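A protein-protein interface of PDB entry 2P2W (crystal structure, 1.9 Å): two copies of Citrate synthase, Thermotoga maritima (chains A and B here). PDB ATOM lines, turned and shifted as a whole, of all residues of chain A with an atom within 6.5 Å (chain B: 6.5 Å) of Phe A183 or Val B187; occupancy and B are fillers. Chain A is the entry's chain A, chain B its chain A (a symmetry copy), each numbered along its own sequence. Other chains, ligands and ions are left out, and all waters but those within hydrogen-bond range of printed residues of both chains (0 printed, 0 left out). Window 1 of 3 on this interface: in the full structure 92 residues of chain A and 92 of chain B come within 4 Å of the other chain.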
ATOM      1  N   LEU A   6      21.208  18.999 -13.516  1.00  0.00           N
ATOM      2  CA  LEU A   6      19.844  19.518 -13.611  1.00  0.00           C
ATOM      3  C   LEU A   6      18.771  18.482 -13.937  1.00  0.00           C
ATOM      4  O   LEU A   6      17.743  18.815 -14.526  1.00  0.00           O
ATOM      5  CB  LEU A   6      19.773  20.642 -14.650  1.00  0.00           C
ATOM      6  CG  LEU A   6      20.542  21.931 -14.346  1.00  0.00           C
ATOM      7  CD1 LEU A   6      20.300  22.937 -15.469  1.00  0.00           C
ATOM      8  CD2 LEU A   6      20.087  22.505 -13.009  1.00  0.00           C
ATOM      9  N   ILE A  11      12.952  23.909 -16.748  1.00  0.00           N
ATOM     10  CA  ILE A  11      13.431  25.264 -16.986  1.00  0.00           C
ATOM     11  C   ILE A  11      12.469  26.138 -17.786  1.00  0.00           C
ATOM     12  O   ILE A  11      12.731  27.323 -17.996  1.00  0.00           O
ATOM     13  CB  ILE A  11      14.812  25.229 -17.679  1.00  0.00           C
ATOM     14  CG1 ILE A  11      14.709  24.566 -19.055  1.00  0.00           C
ATOM     15  CG2 ILE A  11      15.793  24.445 -16.818  1.00  0.00           C
ATOM     16  CD1 ILE A  11      14.606  25.536 -20.216  1.00  0.00           C
ATOM     17  N   ASP A 177      12.476  17.865 -26.749  1.00  0.00           N
ATOM     18  CA  ASP A 177      12.478  18.603 -25.492  1.00  0.00           C
ATOM     19  C   ASP A 177      13.778  19.364 -25.209  1.00  0.00           C
ATOM     20  O   ASP A 177      14.446  19.842 -26.128  1.00  0.00           O
ATOM     21  CB  ASP A 177      12.159  17.621 -24.354  1.00  0.00           C
ATOM     22  CG  ASP A 177      11.610  18.305 -23.116  1.00  0.00           C
ATOM     23  OD1 ASP A 177      10.689  19.138 -23.249  1.00  0.00           O
ATOM     24  OD2 ASP A 177      12.096  17.994 -22.008  1.00  0.00           O
ATOM     25  N   ILE A 178      14.143  19.464 -23.933  1.00  0.00           N
ATOM     26  CA  ILE A 178      15.332  20.217 -23.557  1.00  0.00           C
ATOM     27  C   ILE A 178      16.609  19.403 -23.385  1.00  0.00           C
ATOM     28  O   ILE A 178      17.165  19.310 -22.285  1.00  0.00           O
ATOM     29  CB  ILE A 178      15.070  21.035 -22.273  1.00  0.00           C
ATOM     30  CG1 ILE A 178      13.649  21.606 -22.301  1.00  0.00           C
ATOM     31  CG2 ILE A 178      16.072  22.176 -22.174  1.00  0.00           C
ATOM     32  CD1 ILE A 178      13.345  22.514 -23.495  1.00  0.00           C
ATOM     33  N   ASN A 179      17.073  18.817 -24.484  1.00  0.00           N
ATOM     34  CA  ASN A 179      18.302  18.038 -24.474  1.00  0.00           C
ATOM     35  C   ASN A 179      19.452  19.041 -24.384  1.00  0.00           C
ATOM     36  O   ASN A 179      19.234  20.249 -24.482  1.00  0.00           O
ATOM     37  CB  ASN A 179      18.391  17.202 -25.751  1.00  0.00           C
ATOM     38  CG  ASN A 179      18.160  18.028 -26.995  1.00  0.00           C
ATOM     39  OD1 ASN A 179      19.069  18.681 -27.500  1.00  0.00           O
ATOM     40  ND2 ASN A 179      16.925  18.020 -27.485  1.00  0.00           N
ATOM     41  N   ALA A 180      20.672  18.551 -24.200  1.00  0.00           N
ATOM     42  CA  ALA A 180      21.831  19.429 -24.062  1.00  0.00           C
ATOM     43  C   ALA A 180      22.004  20.494 -25.146  1.00  0.00           C
ATOM     44  O   ALA A 180      22.274  21.650 -24.828  1.00  0.00           O
ATOM     45  CB  ALA A 180      23.106  18.598 -23.944  1.00  0.00           C
ATOM     46  N   SER A 181      21.862  20.124 -26.417  1.00  0.00           N
ATOM     47  CA  SER A 181      22.040  21.110 -27.485  1.00  0.00           C
ATOM     48  C   SER A 181      20.896  22.127 -27.524  1.00  0.00           C
ATOM     49  O   SER A 181      21.127  23.319 -27.731  1.00  0.00           O
ATOM     50  CB  SER A 181      22.208  20.423 -28.852  1.00  0.00           C
ATOM     51  OG  SER A 181      21.062  19.679 -29.238  1.00  0.00           O
ATOM     52  N   THR A 182      19.663  21.668 -27.327  1.00  0.00           N
ATOM     53  CA  THR A 182      18.526  22.591 -27.311  1.00  0.00           C
ATOM     54  C   THR A 182      18.690  23.520 -26.106  1.00  0.00           C
ATOM     55  O   THR A 182      18.402  24.718 -26.182  1.00  0.00           O
ATOM     56  CB  THR A 182      17.177  21.836 -27.195  1.00  0.00           C
ATOM     57  OG1 THR A 182      16.922  21.134 -28.419  1.00  0.00           O
ATOM     58  CG2 THR A 182      16.019  22.807 -26.914  1.00  0.00           C
ATOM     59  N   PHE A 183      19.177  22.972 -24.998  1.00  0.00           N
ATOM     60  CA  PHE A 183      19.365  23.777 -23.797  1.00  0.00           C
ATOM     61  C   PHE A 183      20.448  24.834 -24.018  1.00  0.00           C
ATOM     62  O   PHE A 183      20.313  25.969 -23.558  1.00  0.00           O
ATOM     63  CB  PHE A 183      19.727  22.886 -22.607  1.00  0.00           C
ATOM     64  CG  PHE A 183      19.706  23.606 -21.285  1.00  0.00           C
ATOM     65  CD1 PHE A 183      18.640  24.441 -20.948  1.00  0.00           C
ATOM     66  CD2 PHE A 183      20.729  23.424 -20.364  1.00  0.00           C
ATOM     67  CE1 PHE A 183      18.593  25.082 -19.713  1.00  0.00           C
ATOM     68  CE2 PHE A 183      20.694  24.062 -19.119  1.00  0.00           C
ATOM     69  CZ  PHE A 183      19.621  24.892 -18.797  1.00  0.00           C
ATOM     70  N   ALA A 184      21.519  24.461 -24.715  1.00  0.00           N
ATOM     71  CA  ALA A 184      22.604  25.401 -25.008  1.00  0.00           C
ATOM     72  C   ALA A 184      22.049  26.569 -25.829  1.00  0.00           C
ATOM     73  O   ALA A 184      22.373  27.731 -25.584  1.00  0.00           O
ATOM     74  CB  ALA A 184      23.721  24.692 -25.782  1.00  0.00           C
ATOM     75  N   ALA A 185      21.209  26.249 -26.807  1.00  0.00           N
ATOM     76  CA  ALA A 185      20.605  27.276 -27.649  1.00  0.00           C
ATOM     77  C   ALA A 185      19.726  28.195 -26.807  1.00  0.00           C
ATOM     78  O   ALA A 185      19.674  29.405 -27.045  1.00  0.00           O
ATOM     79  CB  ALA A 185      19.774  26.628 -28.760  1.00  0.00           C
ATOM     80  N   LEU A 186      19.032  27.622 -25.827  1.00  0.00           N
ATOM     81  CA  LEU A 186      18.154  28.412 -24.966  1.00  0.00           C
ATOM     82  C   LEU A 186      18.935  29.335 -24.035  1.00  0.00           C
ATOM     83  O   LEU A 186      18.540  30.482 -23.823  1.00  0.00           O
ATOM     84  CB  LEU A 186      17.240  27.495 -24.143  1.00  0.00           C
ATOM     85  CG  LEU A 186      16.196  26.704 -24.937  1.00  0.00           C
ATOM     86  CD1 LEU A 186      15.335  25.885 -23.976  1.00  0.00           C
ATOM     87  CD2 LEU A 186      15.330  27.667 -25.751  1.00  0.00           C
ATOM     88  N   VAL A 187      20.032  28.838 -23.471  1.00  0.00           N
ATOM     89  CA  VAL A 187      20.849  29.663 -22.582  1.00  0.00           C
ATOM     90  C   VAL A 187      21.346  30.882 -23.352  1.00  0.00           C
ATOM     91  O   VAL A 187      21.268  32.016 -22.873  1.00  0.00           O
ATOM     92  CB  VAL A 187      22.064  28.877 -22.030  1.00  0.00           C
ATOM     93  CG1 VAL A 187      23.016  29.828 -21.296  1.00  0.00           C
ATOM     94  CG2 VAL A 187      21.581  27.794 -21.076  1.00  0.00           C
ATOM     95  N   ILE A 188      21.845  30.642 -24.561  1.00  0.00           N
ATOM     96  CA  ILE A 188      22.341  31.723 -25.397  1.00  0.00           C
ATOM     97  C   ILE A 188      21.187  32.630 -25.810  1.00  0.00           C
ATOM     98  O   ILE A 188      21.311  33.854 -25.783  1.00  0.00           O
ATOM     99  CB  ILE A 188      23.054  31.161 -26.646  1.00  0.00           C
ATOM    100  CG1 ILE A 188      24.308  30.403 -26.204  1.00  0.00           C
ATOM    101  CG2 ILE A 188      23.407  32.296 -27.612  1.00  0.00           C
ATOM    102  CD1 ILE A 188      24.930  29.530 -27.273  1.00  0.00           C
ATOM    103  N   ALA A 205      27.367  21.678 -28.665  1.00  0.00           N
ATOM    104  CA  ALA A 205      26.887  20.694 -27.701  1.00  0.00           C
ATOM    105  C   ALA A 205      26.526  19.372 -28.379  1.00  0.00           C
ATOM    106  O   ALA A 205      26.840  18.293 -27.869  1.00  0.00           O
ATOM    107  CB  ALA A 205      25.673  21.239 -26.965  1.00  0.00           C
ATOM    108  N   TRP A 329      15.637  23.149 -32.512  1.00  0.00           N
ATOM    109  CA  TRP A 329      16.389  24.184 -31.806  1.00  0.00           C
ATOM    110  C   TRP A 329      15.727  25.550 -31.994  1.00  0.00           C
ATOM    111  O   TRP A 329      15.449  26.250 -31.024  1.00  0.00           O
ATOM    112  CB  TRP A 329      17.828  24.278 -32.326  1.00  0.00           C
ATOM    113  CG  TRP A 329      18.736  23.124 -31.975  1.00  0.00           C
ATOM    114  CD1 TRP A 329      18.627  22.278 -30.901  1.00  0.00           C
ATOM    115  CD2 TRP A 329      19.936  22.744 -32.663  1.00  0.00           C
ATOM    116  NE1 TRP A 329      19.688  21.399 -30.880  1.00  0.00           N
ATOM    117  CE2 TRP A 329      20.506  21.663 -31.949  1.00  0.00           C
ATOM    118  CE3 TRP A 329      20.588  23.217 -33.812  1.00  0.00           C
ATOM    119  CZ2 TRP A 329      21.698  21.043 -32.349  1.00  0.00           C
ATOM    120  CZ3 TRP A 329      21.776  22.602 -34.209  1.00  0.00           C
ATOM    121  CH2 TRP A 329      22.317  21.526 -33.477  1.00  0.00           C
ATOM    122  N   ILE A 343      18.855  33.112 -18.299  1.00  0.00           N
ATOM    123  CA  ILE A 343      19.195  31.895 -17.566  1.00  0.00           C
ATOM    124  C   ILE A 343      20.555  32.167 -16.934  1.00  0.00           C
ATOM    125  O   ILE A 343      21.579  32.272 -17.625  1.00  0.00           O
ATOM    126  CB  ILE A 343      19.252  30.669 -18.505  1.00  0.00           C
ATOM    127  CG1 ILE A 343      17.847  30.397 -19.060  1.00  0.00           C
ATOM    128  CG2 ILE A 343      19.771  29.448 -17.743  1.00  0.00           C
ATOM    129  CD1 ILE A 343      17.795  29.351 -20.173  1.00  0.00           C
ATOM    130  N   LEU B   6      16.499  29.713 -13.683  1.00  0.00           N
ATOM    131  CA  LEU B   6      17.380  28.994 -12.763  1.00  0.00           C
ATOM    132  C   LEU B   6      17.991  29.840 -11.648  1.00  0.00           C
ATOM    133  O   LEU B   6      19.076  29.530 -11.157  1.00  0.00           O
ATOM    134  CB  LEU B   6      18.512  28.309 -13.535  1.00  0.00           C
ATOM    135  CG  LEU B   6      18.124  27.178 -14.493  1.00  0.00           C
ATOM    136  CD1 LEU B   6      19.389  26.594 -15.118  1.00  0.00           C
ATOM    137  CD2 LEU B   6      17.356  26.097 -13.739  1.00  0.00           C
ATOM    138  N   THR B 182      29.365  31.719 -19.221  1.00  0.00           N
ATOM    139  CA  THR B 182      30.120  30.638 -18.582  1.00  0.00           C
ATOM    140  C   THR B 182      29.217  29.404 -18.525  1.00  0.00           C
ATOM    141  O   THR B 182      29.670  28.274 -18.729  1.00  0.00           O
ATOM    142  CB  THR B 182      30.560  31.018 -17.145  1.00  0.00           C
ATOM    143  OG1 THR B 182      31.572  32.032 -17.214  1.00  0.00           O
ATOM    144  CG2 THR B 182      31.113  29.797 -16.392  1.00  0.00           C
ATOM    145  N   PHE B 183      27.931  29.623 -18.268  1.00  0.00           N
ATOM    146  CA  PHE B 183      26.995  28.508 -18.189  1.00  0.00           C
ATOM    147  C   PHE B 183      26.840  27.834 -19.553  1.00  0.00           C
ATOM    148  O   PHE B 183      26.753  26.607 -19.635  1.00  0.00           O
ATOM    149  CB  PHE B 183      25.635  28.987 -17.675  1.00  0.00           C
ATOM    150  CG  PHE B 183      24.687  27.867 -17.341  1.00  0.00           C
ATOM    151  CD1 PHE B 183      25.120  26.770 -16.594  1.00  0.00           C
ATOM    152  CD2 PHE B 183      23.358  27.922 -17.739  1.00  0.00           C
ATOM    153  CE1 PHE B 183      24.240  25.747 -16.248  1.00  0.00           C
ATOM    154  CE2 PHE B 183      22.465  26.902 -17.397  1.00  0.00           C
ATOM    155  CZ  PHE B 183      22.911  25.813 -16.649  1.00  0.00           C
ATOM    156  N   ALA B 184      26.799  28.633 -20.617  1.00  0.00           N
ATOM    157  CA  ALA B 184      26.678  28.092 -21.974  1.00  0.00           C
ATOM    158  C   ALA B 184      27.884  27.192 -22.264  1.00  0.00           C
ATOM    159  O   ALA B 184      27.749  26.107 -22.830  1.00  0.00           O
ATOM    160  CB  ALA B 184      26.612  29.233 -22.993  1.00  0.00           C
ATOM    161  N   ALA B 185      29.066  27.652 -21.871  1.00  0.00           N
ATOM    162  CA  ALA B 185      30.286  26.879 -22.080  1.00  0.00           C
ATOM    163  C   ALA B 185      30.217  25.569 -21.303  1.00  0.00           C
ATOM    164  O   ALA B 185      30.686  24.532 -21.779  1.00  0.00           O
ATOM    165  CB  ALA B 185      31.507  27.690 -21.637  1.00  0.00           C
ATOM    166  N   LEU B 186      29.637  25.617 -20.105  1.00  0.00           N
ATOM    167  CA  LEU B 186      29.527  24.418 -19.276  1.00  0.00           C
ATOM    168  C   LEU B 186      28.536  23.408 -19.849  1.00  0.00           C
ATOM    169  O   LEU B 186      28.792  22.204 -19.824  1.00  0.00           O
ATOM    170  CB  LEU B 186      29.121  24.790 -17.845  1.00  0.00           C
ATOM    171  CG  LEU B 186      30.158  25.578 -17.039  1.00  0.00           C
ATOM    172  CD1 LEU B 186      29.630  25.824 -15.626  1.00  0.00           C
ATOM    173  CD2 LEU B 186      31.475  24.801 -16.996  1.00  0.00           C
ATOM    174  N   VAL B 187      27.403  23.892 -20.353  1.00  0.00           N
ATOM    175  CA  VAL B 187      26.409  22.993 -20.939  1.00  0.00           C
ATOM    176  C   VAL B 187      27.045  22.242 -22.105  1.00  0.00           C
ATOM    177  O   VAL B 187      26.913  21.021 -22.226  1.00  0.00           O
ATOM    178  CB  VAL B 187      25.169  23.768 -21.448  1.00  0.00           C
ATOM    179  CG1 VAL B 187      24.261  22.835 -22.257  1.00  0.00           C
ATOM    180  CG2 VAL B 187      24.400  24.334 -20.262  1.00  0.00           C
ATOM    181  N   ILE B 188      27.752  22.979 -22.956  1.00  0.00           N
ATOM    182  CA  ILE B 188      28.414  22.377 -24.101  1.00  0.00           C
ATOM    183  C   ILE B 188      29.533  21.455 -23.627  1.00  0.00           C
ATOM    184  O   ILE B 188      29.694  20.349 -24.141  1.00  0.00           O
ATOM    185  CB  ILE B 188      28.980  23.466 -25.037  1.00  0.00           C
ATOM    186  CG1 ILE B 188      27.817  24.262 -25.634  1.00  0.00           C
ATOM    187  CG2 ILE B 188      29.836  22.831 -26.137  1.00  0.00           C
ATOM    188  CD1 ILE B 188      28.216  25.558 -26.311  1.00  0.00           C
ATOM    189  N   ALA B 189      30.302  21.906 -22.639  1.00  0.00           N
ATOM    190  CA  ALA B 189      31.398  21.099 -22.108  1.00  0.00           C
ATOM    191  C   ALA B 189      30.911  19.794 -21.464  1.00  0.00           C
ATOM    192  O   ALA B 189      31.624  18.787 -21.488  1.00  0.00           O
ATOM    193  CB  ALA B 189      32.198  21.915 -21.090  1.00  0.00           C
ATOM    194  N   SER B 190      29.705  19.811 -20.896  1.00  0.00           N
ATOM    195  CA  SER B 190      29.166  18.630 -20.222  1.00  0.00           C
ATOM    196  C   SER B 190      28.901  17.443 -21.181  1.00  0.00           C
ATOM    197  O   SER B 190      28.717  16.313 -20.758  1.00  0.00           O
ATOM    198  CB  SER B 190      27.879  19.026 -19.499  1.00  0.00           C
ATOM    199  OG  SER B 190      26.800  19.062 -20.433  1.00  0.00           O
ATOM    200  N   THR B 191      28.851  17.743 -22.500  1.00  0.00           N
ATOM    201  CA  THR B 191      28.679  16.665 -23.496  1.00  0.00           C
ATOM    202  C   THR B 191      30.026  16.047 -23.949  1.00  0.00           C
ATOM    203  O   THR B 191      30.106  15.176 -24.816  1.00  0.00           O
ATOM    204  CB  THR B 191      27.966  17.244 -24.718  1.00  0.00           C
ATOM    205  OG1 THR B 191      28.860  18.124 -25.402  1.00  0.00           O
ATOM    206  CG2 THR B 191      26.715  18.026 -24.305  1.00  0.00           C
ATOM    207  N   LEU B 192      31.086  16.581 -23.336  1.00  0.00           N
ATOM    208  CA  LEU B 192      32.484  16.285 -23.583  1.00  0.00           C
ATOM    209  C   LEU B 192      32.936  16.833 -24.932  1.00  0.00           C
ATOM    210  O   LEU B 192      33.865  16.332 -25.550  1.00  0.00           O
ATOM    211  CB  LEU B 192      32.667  14.764 -23.487  1.00  0.00           C
ATOM    212  CG  LEU B 192      32.615  14.286 -22.031  1.00  0.00           C
ATOM    213  CD1 LEU B 192      33.157  12.869 -21.852  1.00  0.00           C
ATOM    214  CD2 LEU B 192      33.420  15.175 -21.081  1.00  0.00           C
ATOM    215  N   TYR B 336      34.986  21.796 -14.213  1.00  0.00           N
ATOM    216  CA  TYR B 336      33.762  21.009 -14.347  1.00  0.00           C
ATOM    217  C   TYR B 336      33.949  19.603 -14.921  1.00  0.00           C
ATOM    218  O   TYR B 336      33.454  18.623 -14.353  1.00  0.00           O
ATOM    219  CB  TYR B 336      32.749  21.742 -15.219  1.00  0.00           C
ATOM    220  CG  TYR B 336      31.376  21.123 -15.166  1.00  0.00           C
ATOM    221  CD1 TYR B 336      30.520  21.372 -14.089  1.00  0.00           C
ATOM    222  CD2 TYR B 336      30.936  20.263 -16.172  1.00  0.00           C
ATOM    223  CE1 TYR B 336      29.263  20.781 -14.015  1.00  0.00           C
ATOM    224  CE2 TYR B 336      29.680  19.665 -16.108  1.00  0.00           C
ATOM    225  CZ  TYR B 336      28.849  19.929 -15.028  1.00  0.00           C
ATOM    226  OH  TYR B 336      27.605  19.350 -14.959  1.00  0.00           O
ATOM    227  N   LEU B 342      26.570  15.298 -17.514  1.00  0.00           N
ATOM    228  CA  LEU B 342      25.801  15.860 -18.612  1.00  0.00           C
ATOM    229  C   LEU B 342      24.724  16.775 -18.034  1.00  0.00           C
ATOM    230  O   LEU B 342      24.080  16.425 -17.050  1.00  0.00           O
ATOM    231  CB  LEU B 342      25.132  14.737 -19.412  1.00  0.00           C
ATOM    232  CG  LEU B 342      24.224  15.179 -20.563  1.00  0.00           C
ATOM    233  CD1 LEU B 342      25.082  15.616 -21.746  1.00  0.00           C
ATOM    234  CD2 LEU B 342      23.308  14.028 -20.971  1.00  0.00           C
ATOM    235  N   ILE B 343      24.546  17.953 -18.632  1.00  0.00           N
ATOM    236  CA  ILE B 343      23.514  18.884 -18.183  1.00  0.00           C
ATOM    237  C   ILE B 343      22.346  18.689 -19.142  1.00  0.00           C
ATOM    238  O   ILE B 343      22.422  19.038 -20.329  1.00  0.00           O
ATOM    239  CB  ILE B 343      24.023  20.342 -18.209  1.00  0.00           C
ATOM    240  CG1 ILE B 343      25.150  20.499 -17.179  1.00  0.00           C
ATOM    241  CG2 ILE B 343      22.874  21.303 -17.895  1.00  0.00           C
ATOM    242  CD1 ILE B 343      25.895  21.831 -17.251  1.00  0.00           C
ATOM    243  N   ARG B 344      21.265  18.123 -18.617  1.00  0.00           N
ATOM    244  CA  ARG B 344      20.099  17.810 -19.432  1.00  0.00           C
ATOM    245  C   ARG B 344      18.829  17.953 -18.598  1.00  0.00           C
ATOM    246  O   ARG B 344      18.375  16.992 -17.968  1.00  0.00           O
ATOM    247  CB  ARG B 344      20.239  16.365 -19.937  1.00  0.00           C
ATOM    248  CG  ARG B 344      19.485  16.018 -21.223  1.00  0.00           C
ATOM    249  CD  ARG B 344      17.978  16.187 -21.110  1.00  0.00           C
ATOM    250  NE  ARG B 344      17.318  15.647 -22.299  1.00  0.00           N
ATOM    251  CZ  ARG B 344      16.049  15.862 -22.620  1.00  0.00           C
ATOM    252  NH1 ARG B 344      15.278  16.619 -21.842  1.00  0.00           N
ATOM    253  NH2 ARG B 344      15.549  15.312 -23.719  1.00  0.00           N
ATOM    254  N   PRO B 345      18.240  19.158 -18.583  1.00  0.00           N
ATOM    255  CA  PRO B 345      17.018  19.406 -17.817  1.00  0.00           C
ATOM    256  C   PRO B 345      15.796  18.987 -18.628  1.00  0.00           C
ATOM    257  O   PRO B 345      15.889  18.147 -19.520  1.00  0.00           O
ATOM    258  CB  PRO B 345      17.069  20.911 -17.585  1.00  0.00           C
ATOM    259  CG  PRO B 345      17.606  21.400 -18.909  1.00  0.00           C
ATOM    260  CD  PRO B 345      18.729  20.402 -19.210  1.00  0.00           C
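Of chain B, only Phe B183 (3.8 Å), Val B187 (3.8 Å), Ile B343 (3.7 Å) and Pro B345 (3.8 Å) come within 4 Å of Phe A183.
Val B187 touches just these residues of chain A: Ala A180 (3.5 Å) and Phe A183 (3.8 Å).
Of the printed residues of chain B, Ile A343 touches Leu B6 (3.9 Å) and Phe B183 (3.7 Å).
Of the printed residues of chain A, Pro B345 touches Leu A6, Ile A11, Ile A178 and Phe A183.
Leu A186 touches none of the printed residues of chain B.
The nearest residue of chain B that does not touch Phe A183 is Leu B6 (4.1 Å).
The nearest residue of chain A that does not touch Val B187 is Ala A184 (4.02 Å).
The nearest printed residue of chain A that does not touch Pro B345 is Asp A177 (4.5 Å).
CA of Pro B345 touches O of Leu A6, at 3.4 Å.
Leu B6 touches Ile A11.
CG2 of Ile A11 touches CB of Pro B345, at 3.8 Å.
NE of Arg B344 touches CA of Asn A179, at 3.4 Å.
Phe B183 touches Phe A183 (CZ to CE2, 3.8 Å).
CD2 of Phe A183 touches CG2 of Val B187, at 3.8 Å.
Phe A183 touches Pro B345.
Phe B183 touches Val A187.
CG2 of Ile B188 touches N of Ala A205 (3.7 Å).
CD1 of Leu B6 touches CG2 of Ile A343 (3.9 Å).
Leu B6 touches its own counterpart, Leu A6.
Phe B183 touches its own counterpart, Phe A183.
Phe A183 touches Val B187, and with the chains exchanged Val A187 touches Phe B183.
Phe A183 touches Ile B343, and with the chains exchanged Ile A343 touches Phe B183.
9 positions are printed for both chains.
Of the 22 pairs that touch across the chains among the printed residues, 8 have their exchanged pair printed and touching as well.
Among the printed residues, 22 pairs touch across the chains.
Among the printed residues, Asp or Glu carboxylates within 4 Å of a Lys or Arg side-chain nitrogen of the other chain: Asp A177 with Arg B344 (3.5 Å).
The backbone carbonyl oxygen (O) of Asp A177 sits at hydrogen-bond distance from the side-chain amide nitrogen (ND2) of Asn A179 (3.4 Å).
The side-chain amide oxygen of Asn A179 lies within hydrogen-bond range of the side-chain hydroxyl of Ser A181, at 2.8 Å.
The side-chain amide oxygen (OD1) of Asn A179 sits at hydrogen-bond distance from the backbone NH (N) of Thr A182, at 3.1 Å.
The backbone carbonyl oxygen (O) of Val B187 is in hydrogen-bond range of the side-chain hydroxyl (OG) of Ser B190.
OG1 of Thr B191 sits at hydrogen-bond distance from O of Ile B188.
OG of Ser B190 is in hydrogen-bond range of N of Ile B343 (3.1 Å).
OD2 of Asp A177 lies within salt-bridge range of NH1 of Arg B344 (3.5 Å).
The backbone carbonyl oxygen (O) of Ile A178 lies within hydrogen-bond range of the guanidinium group (NH1) of Arg B344, 3.3 Å away.
The side-chain hydroxyl of Thr B191 lies within hydrogen-bond range of the backbone carbonyl oxygen of Ala A205.
The backbone carbonyl oxygen of Pro B345 sits close to the backbone carbonyl oxygen of Ile A178.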
